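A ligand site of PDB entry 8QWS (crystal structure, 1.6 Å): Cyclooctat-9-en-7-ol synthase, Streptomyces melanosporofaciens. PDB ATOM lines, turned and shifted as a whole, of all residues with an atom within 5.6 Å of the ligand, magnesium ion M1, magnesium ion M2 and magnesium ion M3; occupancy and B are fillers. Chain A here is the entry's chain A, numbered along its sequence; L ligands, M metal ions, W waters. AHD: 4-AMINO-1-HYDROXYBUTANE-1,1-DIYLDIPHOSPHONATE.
The side-chain hydroxyl (OH) of Tyr 295 sits at hydrogen-bond distance from an oxygen (O12) of the ligand. An oxygen (O17) of the ligand lies within salt-bridge range of the guanidinium group of Arg 177. The guanidinium group (NE) of Arg 294 is in salt-bridge range of an oxygen (O12) of the ligand (2.8 Å). The backbone carbonyl oxygen (O) of Ile 181 sits at hydrogen-bond distance from a nitrogen (N4) of the ligand, at 2.8 Å. O12 of the ligand is in salt-bridge range of NH2 of Arg 227.
The side-chain carboxylate (OD2) of Asp 110 lies close to the guanidinium group (NH2) of Arg 294, at 3.9 Å. The side-chain amide nitrogen of Asn 220 is in hydrogen-bond range of the side-chain hydroxyl of Tyr 295, at 3.4 Å. NH1 of Arg 227 sits close to OE2 of Glu 228 (3.9 Å). O of Glu 228 lies within hydrogen-bond range of N of Gln 233 (2.9 Å). ND2 of Asn 236 is in hydrogen-bond range of OE1 of Glu 228. NH1 of Arg 177 is in salt-bridge range of OD2 of Asp 180. OD1 of Asp 221 lies within salt-bridge range of NH2 of Arg 177 (3.0 Å). The guanidinium group (NH1) of Arg 294 is in salt-bridge range of the side-chain carboxylate (OD2) of Asp 111 (2.8 Å).
Merely in contact with the ligand: Phe 107 (3.7 Å). Hydrophobic or aromatic side chains that line the ligand: Phe 107, Ile 181 and Tyr 295. Ten residues have an atom within 4 Å of the ligand: Phe 107, Asp 110, Arg 177, Ile 181, Asn 220, Ser 224, Arg 227, Glu 228, Arg 294 and Tyr 295.
Residues that only touch magnesium ion M2: Arg 177 (3.96 Å). The nearest printed residue that does not touch magnesium ion M2 is Asp 221 (4.4 Å).
One residue has an atom within 4 Å of magnesium ion M3: Asp 110. The nearest printed residue that does not touch magnesium ion M3 is Asp 180 (4.1 Å).
Magnesium ion M1 is bound by O15 of the ligand (2.0 Å). Magnesium ion M1 is bound by water W8 (2.1 Å). O11 of the ligand binds magnesium ion M1 (2.1 Å). OD2 of Asp 110 binds magnesium ion M1 (2.1 Å). Magnesium ion M1 is bound by water W6 (2.1 Å). Water W2 is bound to magnesium ion M1, at 2.4 Å. Magnesium ion M1 has six donor atoms within binding distance.
Magnesium ion M2 is bound by an oxygen (O10) of the ligand (2.1 Å), the side-chain amide oxygen of Asn 220 (2.1 Å), the side-chain carboxylate of Glu 228 (2.1 Å), water W5 (2.1 Å), an oxygen (O16) of the ligand (2.1 Å) and the side-chain hydroxyl of Ser 224 (2.3 Å). Magnesium ion M2 has six donor atoms within binding distance.
Magnesium ion M3 is bound by water W1 (2.0 Å), water W2 (2.0 Å), the side-chain carboxylate (OD1) of Asp 110 (2.1 Å), an oxygen (O15) of the ligand (2.1 Å), water W9 (2.1 Å) and water W7 (2.2 Å).
Water W9 lies within hydrogen-bond range of the side-chain carboxylate of Asp 180 and the guanidinium group of Arg 177. Water W1 bridges the backbone carbonyl oxygen of Asp 180 and an oxygen (O17) of the ligand. Water W7 lies within hydrogen-bond range of OD1 of Asp 153 (2.5 Å) and OD1 of Asp 180 (2.9 Å). Water W4 lies within hydrogen-bond range of the side-chain hydroxyl (OH) of Tyr 295 (2.7 Å), an oxygen (O13) of the ligand (2.8 Å) and the side-chain amide nitrogen (ND2) of Asn 220 (3.5 Å).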
ATOM      1  N   PHE A 107     -21.296 -20.367 -12.436  1.00  0.00           N
ATOM      2  CA  PHE A 107     -22.338 -19.332 -12.525  1.00  0.00           C
ATOM      3  C   PHE A 107     -22.813 -18.920 -11.138  1.00  0.00           C
ATOM      4  O   PHE A 107     -23.057 -17.724 -10.887  1.00  0.00           O
ATOM      5  CB  PHE A 107     -23.524 -19.846 -13.346  1.00  0.00           C
ATOM      6  CG  PHE A 107     -23.529 -19.368 -14.758  1.00  0.00           C
ATOM      7  CD1 PHE A 107     -23.831 -18.046 -15.064  1.00  0.00           C
ATOM      8  CD2 PHE A 107     -23.233 -20.239 -15.782  1.00  0.00           C
ATOM      9  CE1 PHE A 107     -23.835 -17.621 -16.362  1.00  0.00           C
ATOM     10  CE2 PHE A 107     -23.222 -19.812 -17.099  1.00  0.00           C
ATOM     11  CZ  PHE A 107     -23.515 -18.498 -17.383  1.00  0.00           C
ATOM     12  N   ASP A 110     -20.084 -16.834  -9.635  1.00  0.00           N
ATOM     13  CA  ASP A 110     -20.051 -15.529 -10.302  1.00  0.00           C
ATOM     14  C   ASP A 110     -21.162 -14.610  -9.790  1.00  0.00           C
ATOM     15  O   ASP A 110     -20.994 -13.398  -9.777  1.00  0.00           O
ATOM     16  CB  ASP A 110     -20.197 -15.742 -11.819  1.00  0.00           C
ATOM     17  CG  ASP A 110     -20.128 -14.434 -12.626  1.00  0.00           C
ATOM     18  OD1 ASP A 110     -19.002 -13.969 -12.809  1.00  0.00           O
ATOM     19  OD2 ASP A 110     -21.201 -13.918 -13.122  1.00  0.00           O
ATOM     20  N   ASP A 111     -22.306 -15.173  -9.395  1.00  0.00           N
ATOM     21  CA  ASP A 111     -23.413 -14.348  -8.924  1.00  0.00           C
ATOM     22  C   ASP A 111     -23.374 -14.046  -7.430  1.00  0.00           C
ATOM     23  O   ASP A 111     -24.125 -13.181  -6.981  1.00  0.00           O
ATOM     24  CB  ASP A 111     -24.753 -15.025  -9.249  1.00  0.00           C
ATOM     25  CG  ASP A 111     -25.133 -14.859 -10.706  1.00  0.00           C
ATOM     26  OD1 ASP A 111     -24.537 -14.006 -11.395  1.00  0.00           O
ATOM     27  OD2 ASP A 111     -26.002 -15.603 -11.159  1.00  0.00           O
ATOM     28  N   PHE A 149     -10.059 -19.657 -11.988  1.00  0.00           N
ATOM     29  CA  PHE A 149     -11.164 -18.797 -12.375  1.00  0.00           C
ATOM     30  C   PHE A 149     -11.900 -18.259 -11.155  1.00  0.00           C
ATOM     31  O   PHE A 149     -12.206 -17.056 -11.098  1.00  0.00           O
ATOM     32  CB  PHE A 149     -12.161 -19.537 -13.275  1.00  0.00           C
ATOM     33  CG  PHE A 149     -13.417 -18.731 -13.509  1.00  0.00           C
ATOM     34  CD1 PHE A 149     -13.441 -17.696 -14.434  1.00  0.00           C
ATOM     35  CD2 PHE A 149     -14.551 -18.968 -12.722  1.00  0.00           C
ATOM     36  CE1 PHE A 149     -14.595 -16.939 -14.608  1.00  0.00           C
ATOM     37  CE2 PHE A 149     -15.686 -18.204 -12.891  1.00  0.00           C
ATOM     38  CZ  PHE A 149     -15.705 -17.195 -13.836  1.00  0.00           C
ATOM     39  N   ASP A 153     -12.245 -14.414 -10.067  1.00  0.00           N
ATOM     40  CA  ASP A 153     -13.499 -13.702  -9.873  1.00  0.00           C
ATOM     41  C   ASP A 153     -13.524 -13.047  -8.501  1.00  0.00           C
ATOM     42  O   ASP A 153     -13.968 -11.893  -8.353  1.00  0.00           O
ATOM     43  CB  ASP A 153     -14.676 -14.658 -10.022  1.00  0.00           C
ATOM     44  CG  ASP A 153     -15.980 -13.990  -9.655  1.00  0.00           C
ATOM     45  OD1 ASP A 153     -16.377 -13.064 -10.391  1.00  0.00           O
ATOM     46  OD2 ASP A 153     -16.598 -14.368  -8.636  1.00  0.00           O
ATOM     47  N   ARG A 177     -10.634 -10.296 -19.984  1.00  0.00           N
ATOM     48  CA  ARG A 177     -11.738 -11.226 -20.151  1.00  0.00           C
ATOM     49  C   ARG A 177     -11.289 -12.610 -20.602  1.00  0.00           C
ATOM     50  O   ARG A 177     -12.074 -13.552 -20.450  1.00  0.00           O
ATOM     51  CB  ARG A 177     -12.762 -10.626 -21.120  1.00  0.00           C
ATOM     52  CG  ARG A 177     -13.486  -9.472 -20.415  1.00  0.00           C
ATOM     53  CD  ARG A 177     -14.413 -10.028 -19.298  1.00  0.00           C
ATOM     54  NE  ARG A 177     -15.821  -9.858 -19.678  1.00  0.00           N
ATOM     55  CZ  ARG A 177     -16.812 -10.558 -19.153  1.00  0.00           C
ATOM     56  NH1 ARG A 177     -16.602 -11.448 -18.186  1.00  0.00           N
ATOM     57  NH2 ARG A 177     -18.038 -10.390 -19.632  1.00  0.00           N
ATOM     58  N   ASP A 180     -11.442 -13.794 -17.231  1.00  0.00           N
ATOM     59  CA  ASP A 180     -12.617 -13.471 -16.415  1.00  0.00           C
ATOM     60  C   ASP A 180     -13.946 -13.958 -17.029  1.00  0.00           C
ATOM     61  O   ASP A 180     -14.912 -14.248 -16.288  1.00  0.00           O
ATOM     62  CB  ASP A 180     -12.689 -11.972 -16.180  1.00  0.00           C
ATOM     63  CG  ASP A 180     -13.927 -11.578 -15.404  1.00  0.00           C
ATOM     64  OD1 ASP A 180     -13.974 -11.821 -14.187  1.00  0.00           O
ATOM     65  OD2 ASP A 180     -14.894 -11.065 -15.999  1.00  0.00           O
ATOM     66  N   ILE A 181     -14.066 -13.998 -18.357  1.00  0.00           N
ATOM     67  CA  ILE A 181     -15.345 -14.518 -18.859  1.00  0.00           C
ATOM     68  C   ILE A 181     -15.427 -16.026 -18.749  1.00  0.00           C
ATOM     69  O   ILE A 181     -16.511 -16.613 -18.921  1.00  0.00           O
ATOM     70  CB  ILE A 181     -15.592 -14.077 -20.308  1.00  0.00           C
ATOM     71  CG1 ILE A 181     -17.114 -14.155 -20.599  1.00  0.00           C
ATOM     72  CG2 ILE A 181     -14.738 -14.938 -21.280  1.00  0.00           C
ATOM     73  CD1 ILE A 181     -17.543 -13.384 -21.733  1.00  0.00           C
ATOM     74  N   GLY A 182     -14.308 -16.687 -18.422  1.00  0.00           N
ATOM     75  CA  GLY A 182     -14.341 -18.118 -18.155  1.00  0.00           C
ATOM     76  C   GLY A 182     -13.934 -18.975 -19.325  1.00  0.00           C
ATOM     77  O   GLY A 182     -13.995 -20.216 -19.236  1.00  0.00           O
ATOM     78  N   ASN A 220     -21.877 -11.630 -24.922  1.00  0.00           N
ATOM     79  CA  ASN A 220     -22.366 -11.595 -23.543  1.00  0.00           C
ATOM     80  C   ASN A 220     -22.549 -10.169 -23.072  1.00  0.00           C
ATOM     81  O   ASN A 220     -23.525  -9.853 -22.368  1.00  0.00           O
ATOM     82  CB  ASN A 220     -21.422 -12.334 -22.603  1.00  0.00           C
ATOM     83  CG  ASN A 220     -21.888 -12.174 -21.164  1.00  0.00           C
ATOM     84  OD1 ASN A 220     -21.409 -11.293 -20.445  1.00  0.00           O
ATOM     85  ND2 ASN A 220     -22.908 -12.953 -20.785  1.00  0.00           N
ATOM     86  N   ASP A 221     -21.598  -9.289 -23.383  1.00  0.00           N
ATOM     87  CA  ASP A 221     -21.640  -7.937 -22.829  1.00  0.00           C
ATOM     88  C   ASP A 221     -22.877  -7.205 -23.317  1.00  0.00           C
ATOM     89  O   ASP A 221     -23.468  -6.401 -22.588  1.00  0.00           O
ATOM     90  CB  ASP A 221     -20.374  -7.150 -23.227  1.00  0.00           C
ATOM     91  CG  ASP A 221     -19.141  -7.587 -22.451  1.00  0.00           C
ATOM     92  OD1 ASP A 221     -19.272  -8.358 -21.506  1.00  0.00           O
ATOM     93  OD2 ASP A 221     -18.046  -7.075 -22.798  1.00  0.00           O
ATOM     94  N   SER A 224     -25.899  -8.676 -21.369  1.00  0.00           N
ATOM     95  CA  SER A 224     -25.868  -8.574 -19.918  1.00  0.00           C
ATOM     96  C   SER A 224     -25.609  -7.152 -19.434  1.00  0.00           C
ATOM     97  O   SER A 224     -25.609  -6.909 -18.209  1.00  0.00           O
ATOM     98  CB  SER A 224     -24.855  -9.574 -19.307  1.00  0.00           C
ATOM     99  OG  SER A 224     -23.529  -9.308 -19.737  1.00  0.00           O
ATOM    100  N   ARG A 227     -28.411  -5.541 -16.881  1.00  0.00           N
ATOM    101  CA  ARG A 227     -28.260  -6.131 -15.554  1.00  0.00           C
ATOM    102  C   ARG A 227     -26.996  -5.634 -14.877  1.00  0.00           C
ATOM    103  O   ARG A 227     -27.027  -5.177 -13.730  1.00  0.00           O
ATOM    104  CB  ARG A 227     -28.203  -7.644 -15.670  1.00  0.00           C
ATOM    105  CG  ARG A 227     -27.565  -8.304 -14.446  1.00  0.00           C
ATOM    106  CD  ARG A 227     -27.926  -9.773 -14.261  1.00  0.00           C
ATOM    107  NE  ARG A 227     -27.531 -10.602 -15.391  1.00  0.00           N
ATOM    108  CZ  ARG A 227     -26.297 -11.018 -15.658  1.00  0.00           C
ATOM    109  NH1 ARG A 227     -25.250 -10.613 -14.944  1.00  0.00           N
ATOM    110  NH2 ARG A 227     -26.088 -11.833 -16.686  1.00  0.00           N
ATOM    111  N   GLU A 228     -25.875  -5.691 -15.596  1.00  0.00           N
ATOM    112  CA  GLU A 228     -24.594  -5.364 -14.980  1.00  0.00           C
ATOM    113  C   GLU A 228     -24.551  -3.907 -14.528  1.00  0.00           C
ATOM    114  O   GLU A 228     -24.146  -3.616 -13.396  1.00  0.00           O
ATOM    115  CB  GLU A 228     -23.476  -5.704 -15.972  1.00  0.00           C
ATOM    116  CG  GLU A 228     -23.324  -7.231 -15.964  1.00  0.00           C
ATOM    117  CD  GLU A 228     -22.447  -7.827 -17.045  1.00  0.00           C
ATOM    118  OE1 GLU A 228     -21.775  -7.074 -17.786  1.00  0.00           O
ATOM    119  OE2 GLU A 228     -22.404  -9.085 -17.074  1.00  0.00           O
ATOM    120  N   GLN A 233     -21.710  -3.221 -11.802  1.00  0.00           N
ATOM    121  CA  GLN A 233     -20.597  -3.997 -12.328  1.00  0.00           C
ATOM    122  C   GLN A 233     -19.985  -3.309 -13.541  1.00  0.00           C
ATOM    123  O   GLN A 233     -20.700  -2.807 -14.401  1.00  0.00           O
ATOM    124  CB  GLN A 233     -21.074  -5.408 -12.673  1.00  0.00           C
ATOM    125  CG  GLN A 233     -21.423  -6.263 -11.448  1.00  0.00           C
ATOM    126  CD  GLN A 233     -22.166  -7.552 -11.765  1.00  0.00           C
ATOM    127  OE1 GLN A 233     -23.216  -7.536 -12.391  1.00  0.00           O
ATOM    128  NE2 GLN A 233     -21.634  -8.684 -11.319  1.00  0.00           N
ATOM    129  N   THR A 235     -17.520  -4.682 -15.643  1.00  0.00           N
ATOM    130  CA  THR A 235     -16.844  -5.595 -16.571  1.00  0.00           C
ATOM    131  C   THR A 235     -17.750  -5.796 -17.789  1.00  0.00           C
ATOM    132  O   THR A 235     -18.387  -6.830 -17.930  1.00  0.00           O
ATOM    133  CB  THR A 235     -16.528  -6.908 -15.871  1.00  0.00           C
ATOM    134  OG1 THR A 235     -15.765  -6.632 -14.685  1.00  0.00           O
ATOM    135  CG2 THR A 235     -15.627  -7.752 -16.751  1.00  0.00           C
ATOM    136  N   ASN A 236     -17.713  -4.814 -18.699  1.00  0.00           N
ATOM    137  CA  ASN A 236     -18.582  -4.859 -19.870  1.00  0.00           C
ATOM    138  C   ASN A 236     -18.061  -3.856 -20.880  1.00  0.00           C
ATOM    139  O   ASN A 236     -17.920  -2.664 -20.568  1.00  0.00           O
ATOM    140  CB  ASN A 236     -20.017  -4.542 -19.447  1.00  0.00           C
ATOM    141  CG  ASN A 236     -21.015  -4.763 -20.583  1.00  0.00           C
ATOM    142  OD1 ASN A 236     -20.873  -4.201 -21.673  1.00  0.00           O
ATOM    143  ND2 ASN A 236     -22.003  -5.641 -20.344  1.00  0.00           N
ATOM    144  N   TRP A 288     -27.745 -19.500 -27.132  1.00  0.00           N
ATOM    145  CA  TRP A 288     -28.166 -19.693 -25.752  1.00  0.00           C
ATOM    146  C   TRP A 288     -28.486 -18.359 -25.083  1.00  0.00           C
ATOM    147  O   TRP A 288     -29.484 -18.258 -24.354  1.00  0.00           O
ATOM    148  CB  TRP A 288     -27.100 -20.445 -24.961  1.00  0.00           C
ATOM    149  CG  TRP A 288     -27.314 -20.476 -23.473  1.00  0.00           C
ATOM    150  CD1 TRP A 288     -28.105 -21.336 -22.791  1.00  0.00           C
ATOM    151  CD2 TRP A 288     -26.693 -19.630 -22.486  1.00  0.00           C
ATOM    152  NE1 TRP A 288     -28.030 -21.084 -21.441  1.00  0.00           N
ATOM    153  CE2 TRP A 288     -27.191 -20.020 -21.227  1.00  0.00           C
ATOM    154  CE3 TRP A 288     -25.797 -18.551 -22.553  1.00  0.00           C
ATOM    155  CZ2 TRP A 288     -26.788 -19.404 -20.035  1.00  0.00           C
ATOM    156  CZ3 TRP A 288     -25.405 -17.923 -21.375  1.00  0.00           C
ATOM    157  CH2 TRP A 288     -25.906 -18.358 -20.126  1.00  0.00           C
ATOM    158  N   ARG A 294     -32.055 -15.178 -18.047  1.00  0.00           N
ATOM    159  CA  ARG A 294     -31.007 -14.487 -17.309  1.00  0.00           C
ATOM    160  C   ARG A 294     -30.734 -13.112 -17.897  1.00  0.00           C
ATOM    161  O   ARG A 294     -30.505 -12.137 -17.174  1.00  0.00           O
ATOM    162  CB  ARG A 294     -29.754 -15.359 -17.295  1.00  0.00           C
ATOM    163  CG  ARG A 294     -28.583 -14.747 -16.611  1.00  0.00           C
ATOM    164  CD  ARG A 294     -27.402 -15.731 -16.574  1.00  0.00           C
ATOM    165  NE  ARG A 294     -26.249 -15.079 -15.965  1.00  0.00           N
ATOM    166  CZ  ARG A 294     -26.018 -15.049 -14.662  1.00  0.00           C
ATOM    167  NH1 ARG A 294     -26.856 -15.603 -13.800  1.00  0.00           N
ATOM    168  NH2 ARG A 294     -24.907 -14.463 -14.214  1.00  0.00           N
ATOM    169  N   TYR A 295     -30.840 -12.990 -19.233  1.00  0.00           N
ATOM    170  CA  TYR A 295     -30.476 -11.771 -19.931  1.00  0.00           C
ATOM    171  C   TYR A 295     -31.683 -10.959 -20.405  1.00  0.00           C
ATOM    172  O   TYR A 295     -31.554 -10.145 -21.326  1.00  0.00           O
ATOM    173  CB  TYR A 295     -29.603 -12.112 -21.129  1.00  0.00           C
ATOM    174  CG  TYR A 295     -28.411 -12.865 -20.690  1.00  0.00           C
ATOM    175  CD1 TYR A 295     -27.474 -12.254 -19.828  1.00  0.00           C
ATOM    176  CD2 TYR A 295     -28.233 -14.184 -21.051  1.00  0.00           C
ATOM    177  CE1 TYR A 295     -26.381 -12.957 -19.381  1.00  0.00           C
ATOM    178  CE2 TYR A 295     -27.149 -14.890 -20.607  1.00  0.00           C
ATOM    179  CZ  TYR A 295     -26.210 -14.258 -19.784  1.00  0.00           C
ATOM    180  OH  TYR A 295     -25.151 -14.970 -19.324  1.00  0.00           O
HETATM  181  C2  AHD L   1     -19.938 -15.873 -16.297  1.00  0.00           C
HETATM  182  C3  AHD L   1     -19.771 -16.696 -17.576  1.00  0.00           C
HETATM  183  C7  AHD L   1     -21.176 -14.985 -16.261  1.00  0.00           C
HETATM  184  C8  AHD L   1     -21.259 -13.833 -17.267  1.00  0.00           C
HETATM  185  O12 AHD L   1     -23.992 -14.024 -17.207  1.00  0.00           O
HETATM  186  P9  AHD L   1     -22.896 -12.995 -16.991  1.00  0.00           P
HETATM  187  O10 AHD L   1     -23.144 -11.859 -17.891  1.00  0.00           O
HETATM  188  O11 AHD L   1     -22.902 -12.542 -15.555  1.00  0.00           O
HETATM  189  P14 AHD L   1     -19.932 -12.596 -16.937  1.00  0.00           P
HETATM  190  O15 AHD L   1     -19.864 -12.399 -15.438  1.00  0.00           O
HETATM  191  O16 AHD L   1     -20.246 -11.307 -17.568  1.00  0.00           O
HETATM  192  O17 AHD L   1     -18.640 -13.126 -17.505  1.00  0.00           O
HETATM  193  O13 AHD L   1     -21.138 -14.186 -18.618  1.00  0.00           O
HETATM  194  N4  AHD L   1     -19.219 -15.830 -18.623  1.00  0.00           N
HETATM  195 MG    MG M   1     -21.423 -12.138 -14.169  1.00  0.00          MG
HETATM  196 MG    MG M   2     -21.870 -10.397 -18.624  1.00  0.00          MG
HETATM  197 MG    MG M   3     -18.223 -12.561 -14.105  1.00  0.00          MG
HETATM  198  O   HOH W   1     -17.293 -13.902 -15.311  1.00  0.00           O
HETATM  199  O   HOH W   2     -19.479 -11.316 -13.073  1.00  0.00           O
HETATM  200  O   HOH W   3     -18.960  -9.073 -16.449  1.00  0.00           O
HETATM  201  O   HOH W   4     -22.771 -16.226 -19.641  1.00  0.00           O
HETATM  202  O   HOH W   5     -20.744  -8.763 -19.311  1.00  0.00           O
HETATM  203  O   HOH W   6     -21.809 -10.127 -14.565  1.00  0.00           O
HETATM  204  O   HOH W   7     -16.429 -12.532 -12.843  1.00  0.00           O
HETATM  205  O   HOH W   8     -22.785 -11.768 -12.672  1.00  0.00           O
HETATM  206  O   HOH W   9     -17.303 -10.896 -15.064  1.00  0.00           O
